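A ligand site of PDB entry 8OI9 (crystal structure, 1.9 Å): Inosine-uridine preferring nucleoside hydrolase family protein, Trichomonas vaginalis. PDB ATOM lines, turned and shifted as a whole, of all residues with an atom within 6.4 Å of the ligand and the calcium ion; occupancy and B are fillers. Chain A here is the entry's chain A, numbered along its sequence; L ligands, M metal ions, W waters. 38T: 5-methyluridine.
Along chain A the residues within 4 Å of the calcium ion span positions 10 to 263.
The backbone NH (N) of His 262 is in hydrogen-bond range of the side-chain carboxylate (OD1) of Asp 14, at 2.9 Å. OH of Tyr 250 is in hydrogen-bond range of NE2 of His 262. OD1 of Asn 176 lies within hydrogen-bond range of N of Phe 183 (3.2 Å). ND1 of His 262 is in hydrogen-bond range of OG1 of Thr 211. The side-chain hydroxyl (OG1) of Thr 249 sits at hydrogen-bond distance from the backbone carbonyl oxygen (O) of Phe 246 (2.6 Å). The side-chain amide nitrogen (ND2) of Asn 184 sits close to the backbone carbonyl oxygen (O) of Thr 142 (3.2 Å). The backbone carbonyl oxygen of Met 167 lies within hydrogen-bond range of the side-chain amide nitrogen of Asn 184, at 3.0 Å. N of Asn 184 sits at hydrogen-bond distance from OE2 of Glu 182 (2.8 Å).
O of Thr 142 binds the calcium ion (2.4 Å). The calcium ion is bound by O2' of the ligand (2.4 Å). The side-chain carboxylate (OD2) of Asp 263 binds the calcium ion, 2.4 Å away. Water W3 is bound to the calcium ion (2.4 Å). OD1 of Asp 10 binds the calcium ion (2.4 Å). OD1 of Asp 15 binds the calcium ion (2.4 Å). The side-chain carboxylate (OD2) of Asp 15 is bound to the calcium ion. An oxygen (O3') of the ligand binds the calcium ion, at 2.5 Å. The calcium ion has eight donor atoms within binding distance.
O5' of the ligand sits at hydrogen-bond distance from OE2 of Glu 182 (2.5 Å). An oxygen (O3') of the ligand sits close to the side-chain sulfur (SD) of Met 167 (3.7 Å). O5' of the ligand lies within hydrogen-bond range of ND2 of Asn 176 (2.9 Å). The side-chain amide nitrogen of Asn 184 sits close to an oxygen (O3') of the ligand (3.2 Å). ND2 of Asn 39 sits close to NAI of the ligand.
Merely in contact with the ligand: Tyr 250, Asp 14, Phe 246, Phe 183 and His 262. Hydrophobic or aromatic side chains that line the ligand: Met 167, Phe 183, Phe 246, Tyr 250 and His 262.
Water W3 lies within hydrogen-bond range of OD1 of Asn 184 and OD2 of Asp 10. Water W4 lies within hydrogen-bond range of an oxygen (OAC) of the ligand (2.7 Å) and the backbone carbonyl oxygen (O) of Asp 10 (2.8 Å). Water W1 bridges the side-chain carboxylate of Asp 14 (2.5 Å) and the backbone NH of His 13 (3.2 Å). Water W2 lies within hydrogen-bond range of the side-chain carboxylate (OD2) of Asp 10 (2.6 Å), the backbone NH (N) of Asn 39 (2.7 Å) and an oxygen (OAC) of the ligand (2.9 Å).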
ATOM      1  N   CYS A   9      26.397 -11.346 -24.758  1.00  0.00           N
ATOM      2  CA  CYS A   9      25.733 -10.319 -23.954  1.00  0.00           C
ATOM      3  C   CYS A   9      24.774 -10.920 -22.931  1.00  0.00           C
ATOM      4  O   CYS A   9      24.581 -12.134 -22.880  1.00  0.00           O
ATOM      5  CB  CYS A   9      25.020  -9.340 -24.881  1.00  0.00           C
ATOM      6  SG  CYS A   9      23.816 -10.158 -25.963  1.00  0.00           S
ATOM      7  N   ASP A  10      24.185 -10.047 -22.097  1.00  0.00           N
ATOM      8  CA  ASP A  10      23.279 -10.433 -21.022  1.00  0.00           C
ATOM      9  C   ASP A  10      22.069  -9.497 -20.938  1.00  0.00           C
ATOM     10  O   ASP A  10      21.864  -8.820 -19.928  1.00  0.00           O
ATOM     11  CB  ASP A  10      24.013 -10.410 -19.671  1.00  0.00           C
ATOM     12  CG  ASP A  10      24.543  -9.037 -19.276  1.00  0.00           C
ATOM     13  OD1 ASP A  10      24.696  -8.168 -20.186  1.00  0.00           O
ATOM     14  OD2 ASP A  10      24.759  -8.827 -18.057  1.00  0.00           O
ATOM     15  N   PRO A  11      21.197  -9.429 -21.965  1.00  0.00           N
ATOM     16  CA  PRO A  11      20.127  -8.442 -21.989  1.00  0.00           C
ATOM     17  C   PRO A  11      19.111  -8.615 -20.860  1.00  0.00           C
ATOM     18  O   PRO A  11      18.663  -9.741 -20.630  1.00  0.00           O
ATOM     19  CB  PRO A  11      19.401  -8.630 -23.329  1.00  0.00           C
ATOM     20  CG  PRO A  11      20.083  -9.787 -24.023  1.00  0.00           C
ATOM     21  CD  PRO A  11      21.222 -10.270 -23.171  1.00  0.00           C
ATOM     22  N   GLY A  12      18.771  -7.536 -20.135  1.00  0.00           N
ATOM     23  CA  GLY A  12      19.491  -6.276 -20.110  1.00  0.00           C
ATOM     24  C   GLY A  12      19.015  -5.283 -21.177  1.00  0.00           C
ATOM     25  O   GLY A  12      19.065  -5.588 -22.364  1.00  0.00           O
ATOM     26  N   HIS A  13      18.593  -4.089 -20.726  1.00  0.00           N
ATOM     27  CA  HIS A  13      18.061  -3.041 -21.593  1.00  0.00           C
ATOM     28  C   HIS A  13      19.146  -2.486 -22.512  1.00  0.00           C
ATOM     29  O   HIS A  13      18.897  -2.223 -23.677  1.00  0.00           O
ATOM     30  CB  HIS A  13      17.449  -1.904 -20.768  1.00  0.00           C
ATOM     31  CG  HIS A  13      16.355  -2.338 -19.856  1.00  0.00           C
ATOM     32  ND1 HIS A  13      16.554  -3.140 -18.747  1.00  0.00           N
ATOM     33  CD2 HIS A  13      15.032  -2.086 -19.893  1.00  0.00           C
ATOM     34  CE1 HIS A  13      15.393  -3.355 -18.147  1.00  0.00           C
ATOM     35  NE2 HIS A  13      14.449  -2.724 -18.827  1.00  0.00           N
ATOM     36  N   ASP A  14      20.344  -2.278 -21.949  1.00  0.00           N
ATOM     37  CA  ASP A  14      21.499  -1.815 -22.689  1.00  0.00           C
ATOM     38  C   ASP A  14      21.832  -2.797 -23.820  1.00  0.00           C
ATOM     39  O   ASP A  14      22.085  -2.381 -24.956  1.00  0.00           O
ATOM     40  CB  ASP A  14      22.713  -1.664 -21.769  1.00  0.00           C
ATOM     41  CG  ASP A  14      22.528  -0.576 -20.733  1.00  0.00           C
ATOM     42  OD1 ASP A  14      22.663   0.622 -21.115  1.00  0.00           O
ATOM     43  OD2 ASP A  14      22.196  -0.910 -19.555  1.00  0.00           O
ATOM     44  N   ASP A  15      21.859  -4.082 -23.486  1.00  0.00           N
ATOM     45  CA  ASP A  15      22.242  -5.115 -24.432  1.00  0.00           C
ATOM     46  C   ASP A  15      21.205  -5.162 -25.554  1.00  0.00           C
ATOM     47  O   ASP A  15      21.566  -5.374 -26.716  1.00  0.00           O
ATOM     48  CB  ASP A  15      22.409  -6.478 -23.763  1.00  0.00           C
ATOM     49  CG  ASP A  15      23.292  -6.481 -22.518  1.00  0.00           C
ATOM     50  OD1 ASP A  15      22.845  -5.990 -21.463  1.00  0.00           O
ATOM     51  OD2 ASP A  15      24.412  -6.981 -22.609  1.00  0.00           O
ATOM     52  N   GLY A  38      24.144 -12.858 -15.625  1.00  0.00           N
ATOM     53  CA  GLY A  38      24.377 -11.527 -15.101  1.00  0.00           C
ATOM     54  C   GLY A  38      23.544 -11.307 -13.838  1.00  0.00           C
ATOM     55  O   GLY A  38      23.531 -12.147 -12.927  1.00  0.00           O
ATOM     56  N   ASN A  39      22.846 -10.167 -13.802  1.00  0.00           N
ATOM     57  CA  ASN A  39      21.819  -9.885 -12.812  1.00  0.00           C
ATOM     58  C   ASN A  39      20.708 -10.931 -12.859  1.00  0.00           C
ATOM     59  O   ASN A  39      20.116 -11.239 -11.822  1.00  0.00           O
ATOM     60  CB  ASN A  39      21.167  -8.521 -13.014  1.00  0.00           C
ATOM     61  CG  ASN A  39      21.664  -7.476 -12.049  1.00  0.00           C
ATOM     62  OD1 ASN A  39      22.242  -7.800 -11.015  1.00  0.00           O
ATOM     63  ND2 ASN A  39      21.420  -6.209 -12.374  1.00  0.00           N
ATOM     64  N   THR A 142      29.350  -7.615 -24.065  1.00  0.00           N
ATOM     65  CA  THR A 142      28.726  -6.558 -23.281  1.00  0.00           C
ATOM     66  C   THR A 142      28.086  -7.098 -21.994  1.00  0.00           C
ATOM     67  O   THR A 142      27.273  -6.416 -21.406  1.00  0.00           O
ATOM     68  CB  THR A 142      27.718  -5.765 -24.116  1.00  0.00           C
ATOM     69  OG1 THR A 142      26.596  -6.589 -24.439  1.00  0.00           O
ATOM     70  CG2 THR A 142      28.323  -5.190 -25.372  1.00  0.00           C
ATOM     71  N   GLY A 143      28.494  -8.283 -21.544  1.00  0.00           N
ATOM     72  CA  GLY A 143      28.178  -8.787 -20.214  1.00  0.00           C
ATOM     73  C   GLY A 143      29.428  -9.368 -19.575  1.00  0.00           C
ATOM     74  O   GLY A 143      30.519  -8.981 -19.933  1.00  0.00           O
ATOM     75  N   MET A 167      32.161  -3.714 -23.838  1.00  0.00           N
ATOM     76  CA  MET A 167      31.723  -2.769 -22.837  1.00  0.00           C
ATOM     77  C   MET A 167      32.078  -3.390 -21.500  1.00  0.00           C
ATOM     78  O   MET A 167      31.561  -4.455 -21.149  1.00  0.00           O
ATOM     79  CB  MET A 167      30.223  -2.513 -22.952  1.00  0.00           C
ATOM     80  CG  MET A 167      29.714  -1.389 -22.060  1.00  0.00           C
ATOM     81  SD  MET A 167      29.545  -1.872 -20.331  1.00  0.00           S
ATOM     82  CE  MET A 167      30.492  -0.569 -19.530  1.00  0.00           C
ATOM     83  N   ASN A 176      30.628   1.264 -10.556  1.00  0.00           N
ATOM     84  CA  ASN A 176      29.194   1.444 -10.375  1.00  0.00           C
ATOM     85  C   ASN A 176      28.715   0.550  -9.243  1.00  0.00           C
ATOM     86  O   ASN A 176      28.398   1.042  -8.166  1.00  0.00           O
ATOM     87  CB  ASN A 176      28.419   1.326 -11.700  1.00  0.00           C
ATOM     88  CG  ASN A 176      28.680   0.106 -12.548  1.00  0.00           C
ATOM     89  OD1 ASN A 176      29.214  -0.906 -12.098  1.00  0.00           O
ATOM     90  ND2 ASN A 176      28.247   0.169 -13.800  1.00  0.00           N
ATOM     91  N   ILE A 177      28.686  -0.768  -9.465  1.00  0.00           N
ATOM     92  CA  ILE A 177      28.122  -1.719  -8.523  1.00  0.00           C
ATOM     93  C   ILE A 177      29.057  -1.906  -7.320  1.00  0.00           C
ATOM     94  O   ILE A 177      28.588  -2.252  -6.237  1.00  0.00           O
ATOM     95  CB  ILE A 177      27.802  -3.037  -9.261  1.00  0.00           C
ATOM     96  CG1 ILE A 177      26.636  -2.834 -10.229  1.00  0.00           C
ATOM     97  CG2 ILE A 177      27.519  -4.182  -8.290  1.00  0.00           C
ATOM     98  CD1 ILE A 177      25.340  -2.429  -9.546  1.00  0.00           C
ATOM     99  N   GLU A 182      33.537  -2.138 -12.265  1.00  0.00           N
ATOM    100  CA  GLU A 182      32.361  -2.139 -13.112  1.00  0.00           C
ATOM    101  C   GLU A 182      31.775  -3.550 -13.150  1.00  0.00           C
ATOM    102  O   GLU A 182      32.509  -4.542 -13.089  1.00  0.00           O
ATOM    103  CB  GLU A 182      32.795  -1.595 -14.477  1.00  0.00           C
ATOM    104  CG  GLU A 182      31.713  -1.557 -15.527  1.00  0.00           C
ATOM    105  CD  GLU A 182      31.459  -2.893 -16.203  1.00  0.00           C
ATOM    106  OE1 GLU A 182      32.465  -3.631 -16.451  1.00  0.00           O
ATOM    107  OE2 GLU A 182      30.271  -3.191 -16.479  1.00  0.00           O
ATOM    108  N   PHE A 183      30.451  -3.608 -13.290  1.00  0.00           N
ATOM    109  CA  PHE A 183      29.661  -4.828 -13.140  1.00  0.00           C
ATOM    110  C   PHE A 183      30.203  -5.988 -13.985  1.00  0.00           C
ATOM    111  O   PHE A 183      30.416  -7.093 -13.477  1.00  0.00           O
ATOM    112  CB  PHE A 183      28.211  -4.532 -13.497  1.00  0.00           C
ATOM    113  CG  PHE A 183      27.262  -5.690 -13.334  1.00  0.00           C
ATOM    114  CD1 PHE A 183      26.949  -6.165 -12.071  1.00  0.00           C
ATOM    115  CD2 PHE A 183      26.730  -6.326 -14.440  1.00  0.00           C
ATOM    116  CE1 PHE A 183      26.078  -7.239 -11.914  1.00  0.00           C
ATOM    117  CE2 PHE A 183      25.856  -7.391 -14.287  1.00  0.00           C
ATOM    118  CZ  PHE A 183      25.546  -7.852 -13.022  1.00  0.00           C
ATOM    119  N   ASN A 184      30.366  -5.749 -15.290  1.00  0.00           N
ATOM    120  CA  ASN A 184      30.766  -6.803 -16.220  1.00  0.00           C
ATOM    121  C   ASN A 184      32.105  -7.449 -15.831  1.00  0.00           C
ATOM    122  O   ASN A 184      32.261  -8.650 -16.021  1.00  0.00           O
ATOM    123  CB  ASN A 184      30.815  -6.310 -17.666  1.00  0.00           C
ATOM    124  CG  ASN A 184      29.431  -5.996 -18.195  1.00  0.00           C
ATOM    125  OD1 ASN A 184      28.428  -6.384 -17.597  1.00  0.00           O
ATOM    126  ND2 ASN A 184      29.368  -5.267 -19.296  1.00  0.00           N
ATOM    127  N   LEU A 208      33.077   2.757 -18.423  1.00  0.00           N
ATOM    128  CA  LEU A 208      32.202   3.763 -17.831  1.00  0.00           C
ATOM    129  C   LEU A 208      32.697   5.165 -18.183  1.00  0.00           C
ATOM    130  O   LEU A 208      31.886   6.084 -18.318  1.00  0.00           O
ATOM    131  CB  LEU A 208      32.140   3.566 -16.306  1.00  0.00           C
ATOM    132  CG  LEU A 208      31.577   2.231 -15.820  1.00  0.00           C
ATOM    133  CD1 LEU A 208      31.385   2.281 -14.303  1.00  0.00           C
ATOM    134  CD2 LEU A 208      30.270   1.871 -16.532  1.00  0.00           C
ATOM    135  N   THR A 211      30.774   5.599 -21.356  1.00  0.00           N
ATOM    136  CA  THR A 211      29.327   5.360 -21.330  1.00  0.00           C
ATOM    137  C   THR A 211      28.613   6.308 -20.374  1.00  0.00           C
ATOM    138  O   THR A 211      27.453   6.638 -20.610  1.00  0.00           O
ATOM    139  CB  THR A 211      29.012   3.893 -21.013  1.00  0.00           C
ATOM    140  OG1 THR A 211      29.394   3.574 -19.670  1.00  0.00           O
ATOM    141  CG2 THR A 211      29.673   2.939 -21.990  1.00  0.00           C
ATOM    142  N   PHE A 246      15.279   2.474 -15.639  1.00  0.00           N
ATOM    143  CA  PHE A 246      16.107   2.603 -14.443  1.00  0.00           C
ATOM    144  C   PHE A 246      16.508   4.063 -14.186  1.00  0.00           C
ATOM    145  O   PHE A 246      17.450   4.314 -13.439  1.00  0.00           O
ATOM    146  CB  PHE A 246      17.345   1.702 -14.574  1.00  0.00           C
ATOM    147  CG  PHE A 246      17.045   0.235 -14.404  1.00  0.00           C
ATOM    148  CD1 PHE A 246      16.615  -0.269 -13.189  1.00  0.00           C
ATOM    149  CD2 PHE A 246      17.167  -0.640 -15.480  1.00  0.00           C
ATOM    150  CE1 PHE A 246      16.334  -1.613 -13.042  1.00  0.00           C
ATOM    151  CE2 PHE A 246      16.896  -1.987 -15.324  1.00  0.00           C
ATOM    152  CZ  PHE A 246      16.482  -2.474 -14.109  1.00  0.00           C
ATOM    153  N   THR A 249      16.517   5.171 -10.424  1.00  0.00           N
ATOM    154  CA  THR A 249      17.607   4.541  -9.708  1.00  0.00           C
ATOM    155  C   THR A 249      18.948   5.203 -10.073  1.00  0.00           C
ATOM    156  O   THR A 249      19.777   5.461  -9.213  1.00  0.00           O
ATOM    157  CB  THR A 249      17.629   3.038  -9.973  1.00  0.00           C
ATOM    158  OG1 THR A 249      17.672   2.820 -11.376  1.00  0.00           O
ATOM    159  CG2 THR A 249      16.421   2.330  -9.403  1.00  0.00           C
ATOM    160  N   TYR A 250      19.148   5.475 -11.362  1.00  0.00           N
ATOM    161  CA  TYR A 250      20.337   6.186 -11.801  1.00  0.00           C
ATOM    162  C   TYR A 250      20.388   7.579 -11.164  1.00  0.00           C
ATOM    163  O   TYR A 250      21.462   8.038 -10.765  1.00  0.00           O
ATOM    164  CB  TYR A 250      20.380   6.248 -13.329  1.00  0.00           C
ATOM    165  CG  TYR A 250      21.046   5.079 -14.009  1.00  0.00           C
ATOM    166  CD1 TYR A 250      22.390   4.816 -13.804  1.00  0.00           C
ATOM    167  CD2 TYR A 250      20.346   4.269 -14.898  1.00  0.00           C
ATOM    168  CE1 TYR A 250      23.027   3.759 -14.441  1.00  0.00           C
ATOM    169  CE2 TYR A 250      20.970   3.208 -15.533  1.00  0.00           C
ATOM    170  CZ  TYR A 250      22.310   2.959 -15.319  1.00  0.00           C
ATOM    171  OH  TYR A 250      22.935   1.920 -15.956  1.00  0.00           O
ATOM    172  N   HIS A 262      24.982   2.028 -22.273  1.00  0.00           N
ATOM    173  CA  HIS A 262      26.332   1.480 -22.221  1.00  0.00           C
ATOM    174  C   HIS A 262      26.634   0.678 -23.493  1.00  0.00           C
ATOM    175  O   HIS A 262      27.351   1.139 -24.367  1.00  0.00           O
ATOM    176  CB  HIS A 262      26.503   0.588 -20.979  1.00  0.00           C
ATOM    177  CG  HIS A 262      26.279   1.231 -19.661  1.00  0.00           C
ATOM    178  ND1 HIS A 262      27.215   2.028 -19.031  1.00  0.00           N
ATOM    179  CD2 HIS A 262      25.246   1.127 -18.810  1.00  0.00           C
ATOM    180  CE1 HIS A 262      26.736   2.409 -17.859  1.00  0.00           C
ATOM    181  NE2 HIS A 262      25.530   1.887 -17.710  1.00  0.00           N
ATOM    182  N   ASP A 263      26.024  -0.508 -23.576  1.00  0.00           N
ATOM    183  CA  ASP A 263      26.464  -1.593 -24.453  1.00  0.00           C
ATOM    184  C   ASP A 263      26.519  -1.202 -25.925  1.00  0.00           C
ATOM    185  O   ASP A 263      27.455  -1.585 -26.622  1.00  0.00           O
ATOM    186  CB  ASP A 263      25.594  -2.831 -24.224  1.00  0.00           C
ATOM    187  CG  ASP A 263      25.764  -3.375 -22.819  1.00  0.00           C
ATOM    188  OD1 ASP A 263      26.610  -2.841 -22.080  1.00  0.00           O
ATOM    189  OD2 ASP A 263      25.039  -4.321 -22.465  1.00  0.00           O
HETATM  190  OAC 38T L   1      23.066  -5.813 -16.002  1.00  0.00           O
HETATM  191  CAM 38T L   1      22.745  -4.652 -15.792  1.00  0.00           C
HETATM  192  NAI 38T L   1      21.615  -4.348 -15.059  1.00  0.00           N
HETATM  193  CAL 38T L   1      21.126  -3.099 -14.740  1.00  0.00           C
HETATM  194  OAB 38T L   1      20.103  -2.982 -14.079  1.00  0.00           O
HETATM  195  CAK 38T L   1      21.913  -1.994 -15.257  1.00  0.00           C
HETATM  196  CAA 38T L   1      21.450  -0.594 -14.958  1.00  0.00           C
HETATM  197  CAG 38T L   1      23.011  -2.261 -15.983  1.00  0.00           C
HETATM  198  NAR 38T L   1      23.446  -3.554 -16.251  1.00  0.00           N
HETATM  199  C1' 38T L   1      24.654  -3.793 -17.084  1.00  0.00           C
HETATM  200  O4' 38T L   1      25.770  -3.202 -16.473  1.00  0.00           O
HETATM  201  C4' 38T L   1      26.788  -2.956 -17.487  1.00  0.00           C
HETATM  202  C5' 38T L   1      27.496  -1.664 -17.167  1.00  0.00           C
HETATM  203  O5' 38T L   1      28.258  -1.777 -15.964  1.00  0.00           O
HETATM  204  C3' 38T L   1      26.051  -2.948 -18.845  1.00  0.00           C
HETATM  205  O3' 38T L   1      26.495  -3.959 -19.740  1.00  0.00           O
HETATM  206  C2' 38T L   1      24.582  -3.150 -18.480  1.00  0.00           C
HETATM  207  O2' 38T L   1      23.984  -4.069 -19.360  1.00  0.00           O
HETATM  208 CA    CA M   1      25.114  -5.806 -20.574  1.00  0.00          CA
HETATM  209  O   HOH W   1      21.318  -3.257 -19.270  1.00  0.00           O
HETATM  210  O   HOH W   2      23.016  -8.701 -16.104  1.00  0.00           O
HETATM  211  O   HOH W   3      25.960  -6.496 -18.415  1.00  0.00           O
HETATM  212  O   HOH W   4      22.593  -6.496 -18.610  1.00  0.00           O
